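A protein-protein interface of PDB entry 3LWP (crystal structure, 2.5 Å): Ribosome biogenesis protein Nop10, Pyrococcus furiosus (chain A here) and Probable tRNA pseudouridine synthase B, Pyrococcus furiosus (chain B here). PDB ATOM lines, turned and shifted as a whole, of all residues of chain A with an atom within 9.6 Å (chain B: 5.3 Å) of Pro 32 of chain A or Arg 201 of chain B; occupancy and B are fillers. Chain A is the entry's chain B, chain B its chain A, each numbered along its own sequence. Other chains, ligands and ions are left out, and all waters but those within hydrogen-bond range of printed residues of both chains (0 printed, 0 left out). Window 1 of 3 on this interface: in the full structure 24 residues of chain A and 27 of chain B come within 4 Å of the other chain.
Printed residues of chain B within 4 Å of Ile 5 of chain A: Glu 199 (2.9 Å). Gly 12 of chain A touches none of the printed residues of chain B. Of the printed residues of chain B, Tyr 14 of chain A touches Val 111 (3.5 Å), Arg 201 (3.1 Å), Thr 203 (3.6 Å) and Glu 210 (2.5 Å). Of the printed residues of chain B, Pro 32 of chain A touches Asp 52 (3.3 Å), Lys 53 (3.6 Å), Pro 54 (3.97 Å), Pro 55 (3.7 Å), Ser 86 (3.8 Å) and Arg 201 (3.6 Å). Of the printed residues of chain B, Pro 33 of chain A touches Pro 54 (3.6 Å). Of the printed residues of chain A, Pro 55 of chain B touches Phe 3, Pro 32 and Arg 34. Of chain A, only His 31 (3.0 Å) and Pro 32 (3.8 Å) come within 4 Å of Ser 86 of chain B. Printed residues of chain A within 4 Å of Arg 201 of chain B: Tyr 14 (3.1 Å), Ala 30 (3.5 Å) and Pro 32 (3.6 Å). Arg 202 of chain B touches none of the printed residues of chain A. Printed residues of chain A within 4 Å of Glu 210 of chain B: Lys 7 (3.4 Å) and Tyr 14 (2.5 Å). The nearest printed residue of chain A that does not touch Thr 203 of chain B is Lys 7 of chain A (6.3 Å).
Among the printed residues, merely in contact across the chains: Pro 32 of chain A with Asp 52 of chain B, Tyr 14 of chain A with Val 111 of chain B, Pro 32 of chain A with Arg 201 of chain B, Pro 32 of chain A with Lys 53 of chain B, Tyr 14 of chain A with Thr 203 of chain B, Pro 33 of chain A with Pro 54 of chain B, Pro 32 of chain A with Pro 55 of chain B, Phe 3 of chain A with Pro 55 of chain B, Pro 32 of chain A with Ser 86 of chain B, His 31 of chain A with Leu 200 of chain B, Phe 3 of chain A with Glu 199 of chain B and Pro 32 of chain A with Pro 54 of chain B.
Of the 15 printed residues of chain A, 10 touch a printed residue of chain B. Printed residues of chain A that touch a printed residue of chain B: Phe 3, Arg 4, Ile 5, Lys 7, Tyr 14, Ala 30, His 31, Pro 32, Pro 33 and Arg 34. Of the 19 printed residues of chain B, 11 touch a printed residue of chain A. Hydrophobic or aromatic side chains of chain B within 4 Å of the printed part of chain A: Pro 54, Pro 55 and Val 111.
The backbone NH (N) of Ser 86 of chain B sits at hydrogen-bond distance from the backbone carbonyl oxygen (O) of Leu 200 of chain B (3.4 Å). OD1 of Asp 52 of chain B lies within hydrogen-bond range of N of Gly 87 of chain B (3.2 Å). The backbone NH (N) of Lys 7 of chain A sits at hydrogen-bond distance from the backbone carbonyl oxygen (O) of Lys 28 of chain A (2.7 Å). The side-chain amino group of Lys 53 of chain B sits at hydrogen-bond distance from the backbone carbonyl oxygen of Val 85 of chain B. O of Ile 5 of chain A lies within hydrogen-bond range of N of Ala 30 of chain A. The backbone NH of Val 111 of chain B is in hydrogen-bond range of the backbone carbonyl oxygen of Arg 201 of chain B (2.9 Å).
The side-chain carboxylate of Glu 199 of chain B is in hydrogen-bond range of the backbone NH of Ile 5 of chain A (2.9 Å). The guanidinium group (NH1) of Arg 201 of chain B is in hydrogen-bond range of the backbone carbonyl oxygen (O) of Ala 30 of chain A, 3.5 Å away. The backbone NH (N) of Arg 4 of chain A lies within hydrogen-bond range of the side-chain carboxylate (OE1) of Glu 199 of chain B, at 3.0 Å. The side-chain carboxylate (OE2) of Glu 199 of chain B sits at hydrogen-bond distance from a ring nitrogen (NE2) of His 31 of chain A, at 2.8 Å. The backbone carbonyl oxygen (O) of Pro 55 of chain B lies within hydrogen-bond range of the guanidinium group (NE) of Arg 34 of chain A (3.1 Å). OE1 of Glu 210 of chain B is in hydrogen-bond range of OH of Tyr 14 of chain A (2.5 Å). The guanidinium group (NE) of Arg 201 of chain B sits at hydrogen-bond distance from the side-chain hydroxyl (OH) of Tyr 14 of chain A, at 3.1 Å. A ring nitrogen (ND1) of His 31 of chain A lies within hydrogen-bond range of the side-chain hydroxyl of Ser 86 of chain B (3.0 Å). OE1 of Glu 210 of chain B is in salt-bridge range of NZ of Lys 7 of chain A, 3.4 Å away.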
ATOM      1  N   PHE A   3      -3.225 -32.520   2.064  1.00  0.00           N
ATOM      2  CA  PHE A   3      -3.392 -31.607   0.933  1.00  0.00           C
ATOM      3  C   PHE A   3      -2.306 -31.822  -0.112  1.00  0.00           C
ATOM      4  O   PHE A   3      -1.134 -32.009   0.211  1.00  0.00           O
ATOM      5  CB  PHE A   3      -3.364 -30.155   1.400  1.00  0.00           C
ATOM      6  CG  PHE A   3      -4.585 -29.741   2.170  1.00  0.00           C
ATOM      7  CD1 PHE A   3      -4.462 -29.169   3.435  1.00  0.00           C
ATOM      8  CD2 PHE A   3      -5.856 -29.929   1.634  1.00  0.00           C
ATOM      9  CE1 PHE A   3      -5.584 -28.783   4.153  1.00  0.00           C
ATOM     10  CE2 PHE A   3      -6.984 -29.547   2.342  1.00  0.00           C
ATOM     11  CZ  PHE A   3      -6.849 -28.978   3.606  1.00  0.00           C
ATOM     12  N   ARG A   4      -2.687 -31.780  -1.373  1.00  0.00           N
ATOM     13  CA  ARG A   4      -1.727 -32.109  -2.415  1.00  0.00           C
ATOM     14  C   ARG A   4      -1.101 -30.930  -3.203  1.00  0.00           C
ATOM     15  O   ARG A   4       0.058 -31.013  -3.601  1.00  0.00           O
ATOM     16  CB  ARG A   4      -2.336 -33.149  -3.348  1.00  0.00           C
ATOM     17  CG  ARG A   4      -2.684 -34.451  -2.621  1.00  0.00           C
ATOM     18  CD  ARG A   4      -2.747 -35.596  -3.598  1.00  0.00           C
ATOM     19  NE  ARG A   4      -1.514 -35.650  -4.388  1.00  0.00           N
ATOM     20  CZ  ARG A   4      -1.423 -36.185  -5.600  1.00  0.00           C
ATOM     21  NH1 ARG A   4      -2.493 -36.717  -6.173  1.00  0.00           N
ATOM     22  NH2 ARG A   4      -0.263 -36.184  -6.237  1.00  0.00           N
ATOM     23  N   ILE A   5      -1.860 -29.856  -3.443  1.00  0.00           N
ATOM     24  CA  ILE A   5      -1.374 -28.701  -4.205  1.00  0.00           C
ATOM     25  C   ILE A   5      -0.213 -28.018  -3.463  1.00  0.00           C
ATOM     26  O   ILE A   5      -0.335 -27.642  -2.294  1.00  0.00           O
ATOM     27  CB  ILE A   5      -2.504 -27.675  -4.444  1.00  0.00           C
ATOM     28  CG1 ILE A   5      -3.646 -28.287  -5.253  1.00  0.00           C
ATOM     29  CG2 ILE A   5      -1.978 -26.369  -5.119  1.00  0.00           C
ATOM     30  CD1 ILE A   5      -4.759 -27.258  -5.577  1.00  0.00           C
ATOM     31  N   ARG A   6       0.917 -27.870  -4.139  1.00  0.00           N
ATOM     32  CA  ARG A   6       2.083 -27.240  -3.536  1.00  0.00           C
ATOM     33  C   ARG A   6       2.545 -25.987  -4.309  1.00  0.00           C
ATOM     34  O   ARG A   6       2.076 -25.735  -5.424  1.00  0.00           O
ATOM     35  CB  ARG A   6       3.205 -28.264  -3.446  1.00  0.00           C
ATOM     36  CG  ARG A   6       2.784 -29.545  -2.773  1.00  0.00           C
ATOM     37  CD  ARG A   6       3.958 -30.570  -2.730  1.00  0.00           C
ATOM     38  NE  ARG A   6       5.039 -30.067  -1.886  1.00  0.00           N
ATOM     39  CZ  ARG A   6       5.057 -30.164  -0.562  1.00  0.00           C
ATOM     40  NH1 ARG A   6       4.054 -30.768   0.065  1.00  0.00           N
ATOM     41  NH2 ARG A   6       6.076 -29.659   0.133  1.00  0.00           N
ATOM     42  N   LYS A   7       3.443 -25.192  -3.729  1.00  0.00           N
ATOM     43  CA  LYS A   7       4.110 -24.142  -4.539  1.00  0.00           C
ATOM     44  C   LYS A   7       5.574 -23.759  -4.231  1.00  0.00           C
ATOM     45  O   LYS A   7       6.021 -23.872  -3.091  1.00  0.00           O
ATOM     46  CB  LYS A   7       3.241 -22.903  -4.722  1.00  0.00           C
ATOM     47  CG  LYS A   7       2.661 -22.351  -3.520  1.00  0.00           C
ATOM     48  CD  LYS A   7       2.021 -21.003  -3.872  1.00  0.00           C
ATOM     49  CE  LYS A   7       2.945 -20.113  -4.671  1.00  0.00           C
ATOM     50  NZ  LYS A   7       2.205 -19.012  -5.390  1.00  0.00           N
ATOM     51  N   GLY A  12       6.881 -19.152  -7.566  1.00  0.00           N
ATOM     52  CA  GLY A  12       5.414 -19.168  -7.602  1.00  0.00           C
ATOM     53  C   GLY A  12       4.725 -20.267  -8.464  1.00  0.00           C
ATOM     54  O   GLY A  12       3.498 -20.313  -8.617  1.00  0.00           O
ATOM     55  N   TYR A  14       2.906 -23.555  -9.194  1.00  0.00           N
ATOM     56  CA  TYR A  14       2.088 -24.564  -8.529  1.00  0.00           C
ATOM     57  C   TYR A  14       2.484 -25.912  -9.100  1.00  0.00           C
ATOM     58  O   TYR A  14       2.670 -26.045 -10.301  1.00  0.00           O
ATOM     59  CB  TYR A  14       0.600 -24.282  -8.759  1.00  0.00           C
ATOM     60  CG  TYR A  14       0.054 -23.286  -7.778  1.00  0.00           C
ATOM     61  CD1 TYR A  14      -0.102 -21.938  -8.121  1.00  0.00           C
ATOM     62  CD2 TYR A  14      -0.266 -23.678  -6.488  1.00  0.00           C
ATOM     63  CE1 TYR A  14      -0.578 -21.021  -7.209  1.00  0.00           C
ATOM     64  CE2 TYR A  14      -0.727 -22.774  -5.571  1.00  0.00           C
ATOM     65  CZ  TYR A  14      -0.880 -21.451  -5.931  1.00  0.00           C
ATOM     66  OH  TYR A  14      -1.365 -20.588  -4.991  1.00  0.00           O
ATOM     67  N   LYS A  28       6.319 -25.884  -1.002  1.00  0.00           N
ATOM     68  CA  LYS A  28       5.553 -25.873   0.233  1.00  0.00           C
ATOM     69  C   LYS A  28       4.068 -26.059  -0.037  1.00  0.00           C
ATOM     70  O   LYS A  28       3.561 -25.695  -1.101  1.00  0.00           O
ATOM     71  CB  LYS A  28       5.803 -24.563   0.990  1.00  0.00           C
ATOM     72  CG  LYS A  28       6.640 -24.742   2.257  1.00  0.00           C
ATOM     73  CD  LYS A  28       7.881 -23.865   2.285  1.00  0.00           C
ATOM     74  CE  LYS A  28       9.123 -24.678   1.901  1.00  0.00           C
ATOM     75  NZ  LYS A  28      10.398 -23.928   2.112  1.00  0.00           N
ATOM     76  N   VAL A  29       3.375 -26.635   0.935  1.00  0.00           N
ATOM     77  CA  VAL A  29       1.933 -26.768   0.865  1.00  0.00           C
ATOM     78  C   VAL A  29       1.243 -25.432   0.556  1.00  0.00           C
ATOM     79  O   VAL A  29       1.357 -24.495   1.324  1.00  0.00           O
ATOM     80  CB  VAL A  29       1.376 -27.339   2.188  1.00  0.00           C
ATOM     81  CG1 VAL A  29      -0.141 -27.384   2.144  1.00  0.00           C
ATOM     82  CG2 VAL A  29       1.960 -28.725   2.445  1.00  0.00           C
ATOM     83  N   ALA A  30       0.496 -25.368  -0.543  1.00  0.00           N
ATOM     84  CA  ALA A  30      -0.228 -24.150  -0.937  1.00  0.00           C
ATOM     85  C   ALA A  30      -1.231 -23.553   0.064  1.00  0.00           C
ATOM     86  O   ALA A  30      -1.410 -22.335   0.108  1.00  0.00           O
ATOM     87  CB  ALA A  30      -0.918 -24.363  -2.270  1.00  0.00           C
ATOM     88  N   HIS A  31      -1.918 -24.384   0.836  1.00  0.00           N
ATOM     89  CA  HIS A  31      -2.981 -23.875   1.720  1.00  0.00           C
ATOM     90  C   HIS A  31      -2.449 -23.262   3.012  1.00  0.00           C
ATOM     91  O   HIS A  31      -1.405 -23.668   3.501  1.00  0.00           O
ATOM     92  CB  HIS A  31      -4.002 -24.970   1.981  1.00  0.00           C
ATOM     93  CG  HIS A  31      -4.542 -25.556   0.714  1.00  0.00           C
ATOM     94  ND1 HIS A  31      -5.698 -25.097   0.113  1.00  0.00           N
ATOM     95  CD2 HIS A  31      -4.042 -26.511  -0.109  1.00  0.00           C
ATOM     96  CE1 HIS A  31      -5.906 -25.772  -1.005  1.00  0.00           C
ATOM     97  NE2 HIS A  31      -4.914 -26.631  -1.166  1.00  0.00           N
ATOM     98  N   PRO A  32      -3.122 -22.218   3.511  1.00  0.00           N
ATOM     99  CA  PRO A  32      -2.728 -21.639   4.792  1.00  0.00           C
ATOM    100  C   PRO A  32      -3.096 -22.586   5.932  1.00  0.00           C
ATOM    101  O   PRO A  32      -4.114 -23.262   5.843  1.00  0.00           O
ATOM    102  CB  PRO A  32      -3.587 -20.362   4.897  1.00  0.00           C
ATOM    103  CG  PRO A  32      -4.311 -20.222   3.627  1.00  0.00           C
ATOM    104  CD  PRO A  32      -4.272 -21.524   2.910  1.00  0.00           C
ATOM    105  N   PRO A  33      -2.295 -22.610   6.999  1.00  0.00           N
ATOM    106  CA  PRO A  33      -2.642 -23.386   8.201  1.00  0.00           C
ATOM    107  C   PRO A  33      -4.054 -23.059   8.660  1.00  0.00           C
ATOM    108  O   PRO A  33      -4.565 -21.969   8.418  1.00  0.00           O
ATOM    109  CB  PRO A  33      -1.669 -22.866   9.263  1.00  0.00           C
ATOM    110  CG  PRO A  33      -0.605 -22.133   8.531  1.00  0.00           C
ATOM    111  CD  PRO A  33      -1.169 -21.684   7.218  1.00  0.00           C
ATOM    112  N   ARG A  34      -4.674 -24.001   9.344  1.00  0.00           N
ATOM    113  CA  ARG A  34      -5.975 -23.760   9.937  1.00  0.00           C
ATOM    114  C   ARG A  34      -5.864 -22.822  11.116  1.00  0.00           C
ATOM    115  O   ARG A  34      -4.907 -22.881  11.877  1.00  0.00           O
ATOM    116  CB  ARG A  34      -6.612 -25.073  10.360  1.00  0.00           C
ATOM    117  CG  ARG A  34      -6.966 -25.941   9.159  1.00  0.00           C
ATOM    118  CD  ARG A  34      -8.120 -26.875   9.472  1.00  0.00           C
ATOM    119  NE  ARG A  34      -8.873 -27.233   8.271  1.00  0.00           N
ATOM    120  CZ  ARG A  34      -8.368 -27.922   7.254  1.00  0.00           C
ATOM    121  NH1 ARG A  34      -7.097 -28.318   7.289  1.00  0.00           N
ATOM    122  NH2 ARG A  34      -9.132 -28.205   6.203  1.00  0.00           N
ATOM    123  N   PHE A  35      -6.848 -21.941  11.237  1.00  0.00           N
ATOM    124  CA  PHE A  35      -6.871 -20.942  12.272  1.00  0.00           C
ATOM    125  C   PHE A  35      -8.153 -21.096  13.053  1.00  0.00           C
ATOM    126  O   PHE A  35      -9.179 -21.439  12.477  1.00  0.00           O
ATOM    127  CB  PHE A  35      -6.844 -19.544  11.643  1.00  0.00           C
ATOM    128  CG  PHE A  35      -6.997 -18.435  12.643  1.00  0.00           C
ATOM    129  CD1 PHE A  35      -5.880 -17.879  13.249  1.00  0.00           C
ATOM    130  CD2 PHE A  35      -8.268 -17.976  13.004  1.00  0.00           C
ATOM    131  CE1 PHE A  35      -6.018 -16.877  14.189  1.00  0.00           C
ATOM    132  CE2 PHE A  35      -8.418 -16.954  13.926  1.00  0.00           C
ATOM    133  CZ  PHE A  35      -7.286 -16.404  14.522  1.00  0.00           C
ATOM    134  N   ASP B  52      -5.776 -14.381   2.681  1.00  0.00           N
ATOM    135  CA  ASP B  52      -5.662 -15.791   2.288  1.00  0.00           C
ATOM    136  C   ASP B  52      -6.547 -16.680   3.196  1.00  0.00           C
ATOM    137  O   ASP B  52      -6.121 -17.077   4.278  1.00  0.00           O
ATOM    138  CB  ASP B  52      -4.215 -16.244   2.420  1.00  0.00           C
ATOM    139  CG  ASP B  52      -3.947 -17.555   1.691  1.00  0.00           C
ATOM    140  OD1 ASP B  52      -4.934 -18.128   1.182  1.00  0.00           O
ATOM    141  OD2 ASP B  52      -2.758 -18.001   1.605  1.00  0.00           O
ATOM    142  N   LYS B  53      -7.776 -16.966   2.762  1.00  0.00           N
ATOM    143  CA  LYS B  53      -8.707 -17.804   3.514  1.00  0.00           C
ATOM    144  C   LYS B  53      -8.193 -19.239   3.678  1.00  0.00           C
ATOM    145  O   LYS B  53      -7.756 -19.840   2.709  1.00  0.00           O
ATOM    146  CB  LYS B  53     -10.057 -17.828   2.799  1.00  0.00           C
ATOM    147  CG  LYS B  53     -10.988 -18.921   3.288  1.00  0.00           C
ATOM    148  CD  LYS B  53     -12.363 -18.843   2.633  1.00  0.00           C
ATOM    149  CE  LYS B  53     -13.311 -19.938   3.161  1.00  0.00           C
ATOM    150  NZ  LYS B  53     -12.625 -21.288   3.252  1.00  0.00           N
ATOM    151  N   PRO B  54      -8.247 -19.796   4.910  1.00  0.00           N
ATOM    152  CA  PRO B  54      -7.869 -21.209   5.087  1.00  0.00           C
ATOM    153  C   PRO B  54      -9.005 -22.125   4.670  1.00  0.00           C
ATOM    154  O   PRO B  54     -10.163 -21.698   4.597  1.00  0.00           O
ATOM    155  CB  PRO B  54      -7.652 -21.351   6.613  1.00  0.00           C
ATOM    156  CG  PRO B  54      -8.279 -20.175   7.240  1.00  0.00           C
ATOM    157  CD  PRO B  54      -8.774 -19.220   6.160  1.00  0.00           C
ATOM    158  N   PRO B  55      -8.684 -23.379   4.373  1.00  0.00           N
ATOM    159  CA  PRO B  55      -9.727 -24.397   4.200  1.00  0.00           C
ATOM    160  C   PRO B  55     -10.384 -24.676   5.564  1.00  0.00           C
ATOM    161  O   PRO B  55      -9.657 -24.763   6.546  1.00  0.00           O
ATOM    162  CB  PRO B  55      -8.927 -25.617   3.775  1.00  0.00           C
ATOM    163  CG  PRO B  55      -7.593 -25.408   4.499  1.00  0.00           C
ATOM    164  CD  PRO B  55      -7.332 -23.951   4.252  1.00  0.00           C
ATOM    165  N   VAL B  85     -12.375 -24.362   0.174  1.00  0.00           N
ATOM    166  CA  VAL B  85     -11.539 -23.636  -0.754  1.00  0.00           C
ATOM    167  C   VAL B  85     -10.662 -22.615  -0.019  1.00  0.00           C
ATOM    168  O   VAL B  85     -11.132 -21.919   0.872  1.00  0.00           O
ATOM    169  CB  VAL B  85     -12.409 -22.977  -1.809  1.00  0.00           C
ATOM    170  CG1 VAL B  85     -11.559 -22.174  -2.777  1.00  0.00           C
ATOM    171  CG2 VAL B  85     -13.243 -24.057  -2.536  1.00  0.00           C
ATOM    172  N   SER B  86      -9.381 -22.561  -0.363  1.00  0.00           N
ATOM    173  CA  SER B  86      -8.477 -21.558   0.215  1.00  0.00           C
ATOM    174  C   SER B  86      -8.235 -20.415  -0.783  1.00  0.00           C
ATOM    175  O   SER B  86      -8.730 -20.449  -1.907  1.00  0.00           O
ATOM    176  CB  SER B  86      -7.123 -22.171   0.553  1.00  0.00           C
ATOM    177  OG  SER B  86      -6.356 -22.277  -0.647  1.00  0.00           O
ATOM    178  N   GLY B  87      -7.478 -19.402  -0.361  1.00  0.00           N
ATOM    179  CA  GLY B  87      -7.024 -18.376  -1.286  1.00  0.00           C
ATOM    180  C   GLY B  87      -7.663 -17.005  -1.166  1.00  0.00           C
ATOM    181  O   GLY B  87      -8.235 -16.625  -0.128  1.00  0.00           O
ATOM    182  N   GLU B 109      -9.268 -16.158 -10.760  1.00  0.00           N
ATOM    183  CA  GLU B 109      -8.427 -17.233 -11.231  1.00  0.00           C
ATOM    184  C   GLU B 109      -8.263 -18.278 -10.127  1.00  0.00           C
ATOM    185  O   GLU B 109      -8.255 -17.949  -8.942  1.00  0.00           O
ATOM    186  CB  GLU B 109      -7.094 -16.720 -11.736  1.00  0.00           C
ATOM    187  CG  GLU B 109      -6.284 -17.766 -12.458  1.00  0.00           C
ATOM    188  CD  GLU B 109      -4.778 -17.746 -12.126  1.00  0.00           C
ATOM    189  OE1 GLU B 109      -4.155 -16.651 -12.031  1.00  0.00           O
ATOM    190  OE2 GLU B 109      -4.211 -18.859 -11.978  1.00  0.00           O
ATOM    191  N   TYR B 110      -8.170 -19.541 -10.544  1.00  0.00           N
ATOM    192  CA  TYR B 110      -8.061 -20.664  -9.631  1.00  0.00           C
ATOM    193  C   TYR B 110      -6.989 -21.655 -10.049  1.00  0.00           C
ATOM    194  O   TYR B 110      -6.724 -21.862 -11.231  1.00  0.00           O
ATOM    195  CB  TYR B 110      -9.382 -21.406  -9.577  1.00  0.00           C
ATOM    196  CG  TYR B 110     -10.545 -20.609  -9.064  1.00  0.00           C
ATOM    197  CD1 TYR B 110     -11.341 -19.868  -9.936  1.00  0.00           C
ATOM    198  CD2 TYR B 110     -10.872 -20.623  -7.699  1.00  0.00           C
ATOM    199  CE1 TYR B 110     -12.437 -19.167  -9.458  1.00  0.00           C
ATOM    200  CE2 TYR B 110     -11.946 -19.897  -7.206  1.00  0.00           C
ATOM    201  CZ  TYR B 110     -12.713 -19.175  -8.086  1.00  0.00           C
ATOM    202  OH  TYR B 110     -13.760 -18.463  -7.603  1.00  0.00           O
ATOM    203  N   VAL B 111      -6.377 -22.273  -9.060  1.00  0.00           N
ATOM    204  CA  VAL B 111      -5.594 -23.462  -9.293  1.00  0.00           C
ATOM    205  C   VAL B 111      -6.460 -24.593  -8.727  1.00  0.00           C
ATOM    206  O   VAL B 111      -6.974 -24.520  -7.582  1.00  0.00           O
ATOM    207  CB  VAL B 111      -4.241 -23.369  -8.589  1.00  0.00           C
ATOM    208  CG1 VAL B 111      -3.410 -24.601  -8.831  1.00  0.00           C
ATOM    209  CG2 VAL B 111      -3.497 -22.142  -9.091  1.00  0.00           C
ATOM    210  N   ALA B 112      -6.676 -25.607  -9.555  1.00  0.00           N
ATOM    211  CA  ALA B 112      -7.646 -26.647  -9.242  1.00  0.00           C
ATOM    212  C   ALA B 112      -7.024 -28.000  -9.413  1.00  0.00           C
ATOM    213  O   ALA B 112      -6.194 -28.203 -10.293  1.00  0.00           O
ATOM    214  CB  ALA B 112      -8.889 -26.512 -10.110  1.00  0.00           C
ATOM    215  N   GLU B 199      -9.530 -30.528  -4.958  1.00  0.00           N
ATOM    216  CA  GLU B 199      -8.804 -29.432  -4.310  1.00  0.00           C
ATOM    217  C   GLU B 199      -8.961 -28.148  -5.102  1.00  0.00           C
ATOM    218  O   GLU B 199      -8.783 -28.135  -6.324  1.00  0.00           O
ATOM    219  CB  GLU B 199      -7.310 -29.784  -4.177  1.00  0.00           C
ATOM    220  CG  GLU B 199      -6.609 -29.121  -3.020  1.00  0.00           C
ATOM    221  CD  GLU B 199      -5.368 -29.877  -2.518  1.00  0.00           C
ATOM    222  OE1 GLU B 199      -5.388 -31.129  -2.381  1.00  0.00           O
ATOM    223  OE2 GLU B 199      -4.363 -29.198  -2.219  1.00  0.00           O
ATOM    224  N   LEU B 200      -9.257 -27.063  -4.396  1.00  0.00           N
ATOM    225  CA  LEU B 200      -9.443 -25.761  -5.039  1.00  0.00           C
ATOM    226  C   LEU B 200      -8.774 -24.606  -4.279  1.00  0.00           C
ATOM    227  O   LEU B 200      -8.842 -24.535  -3.061  1.00  0.00           O
ATOM    228  CB  LEU B 200     -10.937 -25.480  -5.276  1.00  0.00           C
ATOM    229  CG  LEU B 200     -11.278 -24.260  -6.141  1.00  0.00           C
ATOM    230  CD1 LEU B 200     -10.699 -24.406  -7.538  1.00  0.00           C
ATOM    231  CD2 LEU B 200     -12.785 -24.002  -6.204  1.00  0.00           C
ATOM    232  N   ARG B 201      -8.128 -23.698  -5.005  1.00  0.00           N
ATOM    233  CA  ARG B 201      -7.514 -22.507  -4.389  1.00  0.00           C
ATOM    234  C   ARG B 201      -7.649 -21.291  -5.303  1.00  0.00           C
ATOM    235  O   ARG B 201      -7.211 -21.327  -6.451  1.00  0.00           O
ATOM    236  CB  ARG B 201      -6.031 -22.761  -4.047  1.00  0.00           C
ATOM    237  CG  ARG B 201      -5.182 -21.493  -3.907  1.00  0.00           C
ATOM    238  CD  ARG B 201      -3.917 -21.737  -3.087  1.00  0.00           C
ATOM    239  NE  ARG B 201      -3.344 -20.472  -2.633  1.00  0.00           N
ATOM    240  CZ  ARG B 201      -3.544 -19.925  -1.432  1.00  0.00           C
ATOM    241  NH1 ARG B 201      -4.292 -20.525  -0.506  1.00  0.00           N
ATOM    242  NH2 ARG B 201      -2.985 -18.756  -1.142  1.00  0.00           N
ATOM    243  N   ARG B 202      -8.276 -20.229  -4.815  1.00  0.00           N
ATOM    244  CA  ARG B 202      -8.407 -19.014  -5.618  1.00  0.00           C
ATOM    245  C   ARG B 202      -7.121 -18.202  -5.575  1.00  0.00           C
ATOM    246  O   ARG B 202      -6.708 -17.756  -4.514  1.00  0.00           O
ATOM    247  CB  ARG B 202      -9.547 -18.158  -5.125  1.00  0.00           C
ATOM    248  CG  ARG B 202     -10.034 -17.195  -6.156  1.00  0.00           C
ATOM    249  CD  ARG B 202     -10.721 -16.050  -5.494  1.00  0.00           C
ATOM    250  NE  ARG B 202     -12.151 -16.088  -5.697  1.00  0.00           N
ATOM    251  CZ  ARG B 202     -13.030 -15.626  -4.822  1.00  0.00           C
ATOM    252  NH1 ARG B 202     -12.624 -15.118  -3.677  1.00  0.00           N
ATOM    253  NH2 ARG B 202     -14.319 -15.678  -5.098  1.00  0.00           N
ATOM    254  N   THR B 203      -6.484 -18.036  -6.726  1.00  0.00           N
ATOM    255  CA  THR B 203      -5.210 -17.354  -6.770  1.00  0.00           C
ATOM    256  C   THR B 203      -5.347 -15.874  -7.111  1.00  0.00           C
ATOM    257  O   THR B 203      -4.374 -15.130  -7.024  1.00  0.00           O
ATOM    258  CB  THR B 203      -4.245 -17.973  -7.795  1.00  0.00           C
ATOM    259  OG1 THR B 203      -4.891 -18.076  -9.061  1.00  0.00           O
ATOM    260  CG2 THR B 203      -3.765 -19.325  -7.337  1.00  0.00           C
ATOM    261  N   GLU B 210      -1.864 -13.075  -5.725  1.00  0.00           N
ATOM    262  CA  GLU B 210      -0.955 -13.674  -4.762  1.00  0.00           C
ATOM    263  C   GLU B 210       0.381 -12.950  -4.637  1.00  0.00           C
ATOM    264  O   GLU B 210       1.420 -13.482  -4.994  1.00  0.00           O
ATOM    265  CB  GLU B 210      -0.689 -15.124  -5.119  1.00  0.00           C
ATOM    266  CG  GLU B 210      -1.766 -16.099  -4.720  1.00  0.00           C
ATOM    267  CD  GLU B 210      -1.218 -17.519  -4.623  1.00  0.00           C
ATOM    268  OE1 GLU B 210      -1.084 -18.191  -5.679  1.00  0.00           O
ATOM    269  OE2 GLU B 210      -0.895 -17.941  -3.486  1.00  0.00           O
ATOM    270  N   LEU B 214      -0.918 -10.627   0.205  1.00  0.00           N
ATOM    271  CA  LEU B 214      -1.726 -11.783   0.557  1.00  0.00           C
ATOM    272  C   LEU B 214      -1.399 -12.263   1.982  1.00  0.00           C
ATOM    273  O   LEU B 214      -0.337 -12.838   2.237  1.00  0.00           O
ATOM    274  CB  LEU B 214      -1.475 -12.911  -0.423  1.00  0.00           C
ATOM    275  CG  LEU B 214      -2.574 -13.956  -0.369  1.00  0.00           C
ATOM    276  CD1 LEU B 214      -3.866 -13.218  -0.665  1.00  0.00           C
ATOM    277  CD2 LEU B 214      -2.279 -15.017  -1.392  1.00  0.00           C
ATOM    278  N   THR B 216      -2.260 -14.323   5.638  1.00  0.00           N
ATOM    279  CA  THR B 216      -3.011 -15.301   6.444  1.00  0.00           C
ATOM    280  C   THR B 216      -3.622 -14.695   7.704  1.00  0.00           C
ATOM    281  O   THR B 216      -3.278 -13.589   8.098  1.00  0.00           O
ATOM    282  CB  THR B 216      -2.127 -16.454   6.929  1.00  0.00           C
ATOM    283  OG1 THR B 216      -1.212 -15.957   7.900  1.00  0.00           O
ATOM    284  CG2 THR B 216      -1.358 -17.135   5.762  1.00  0.00           C
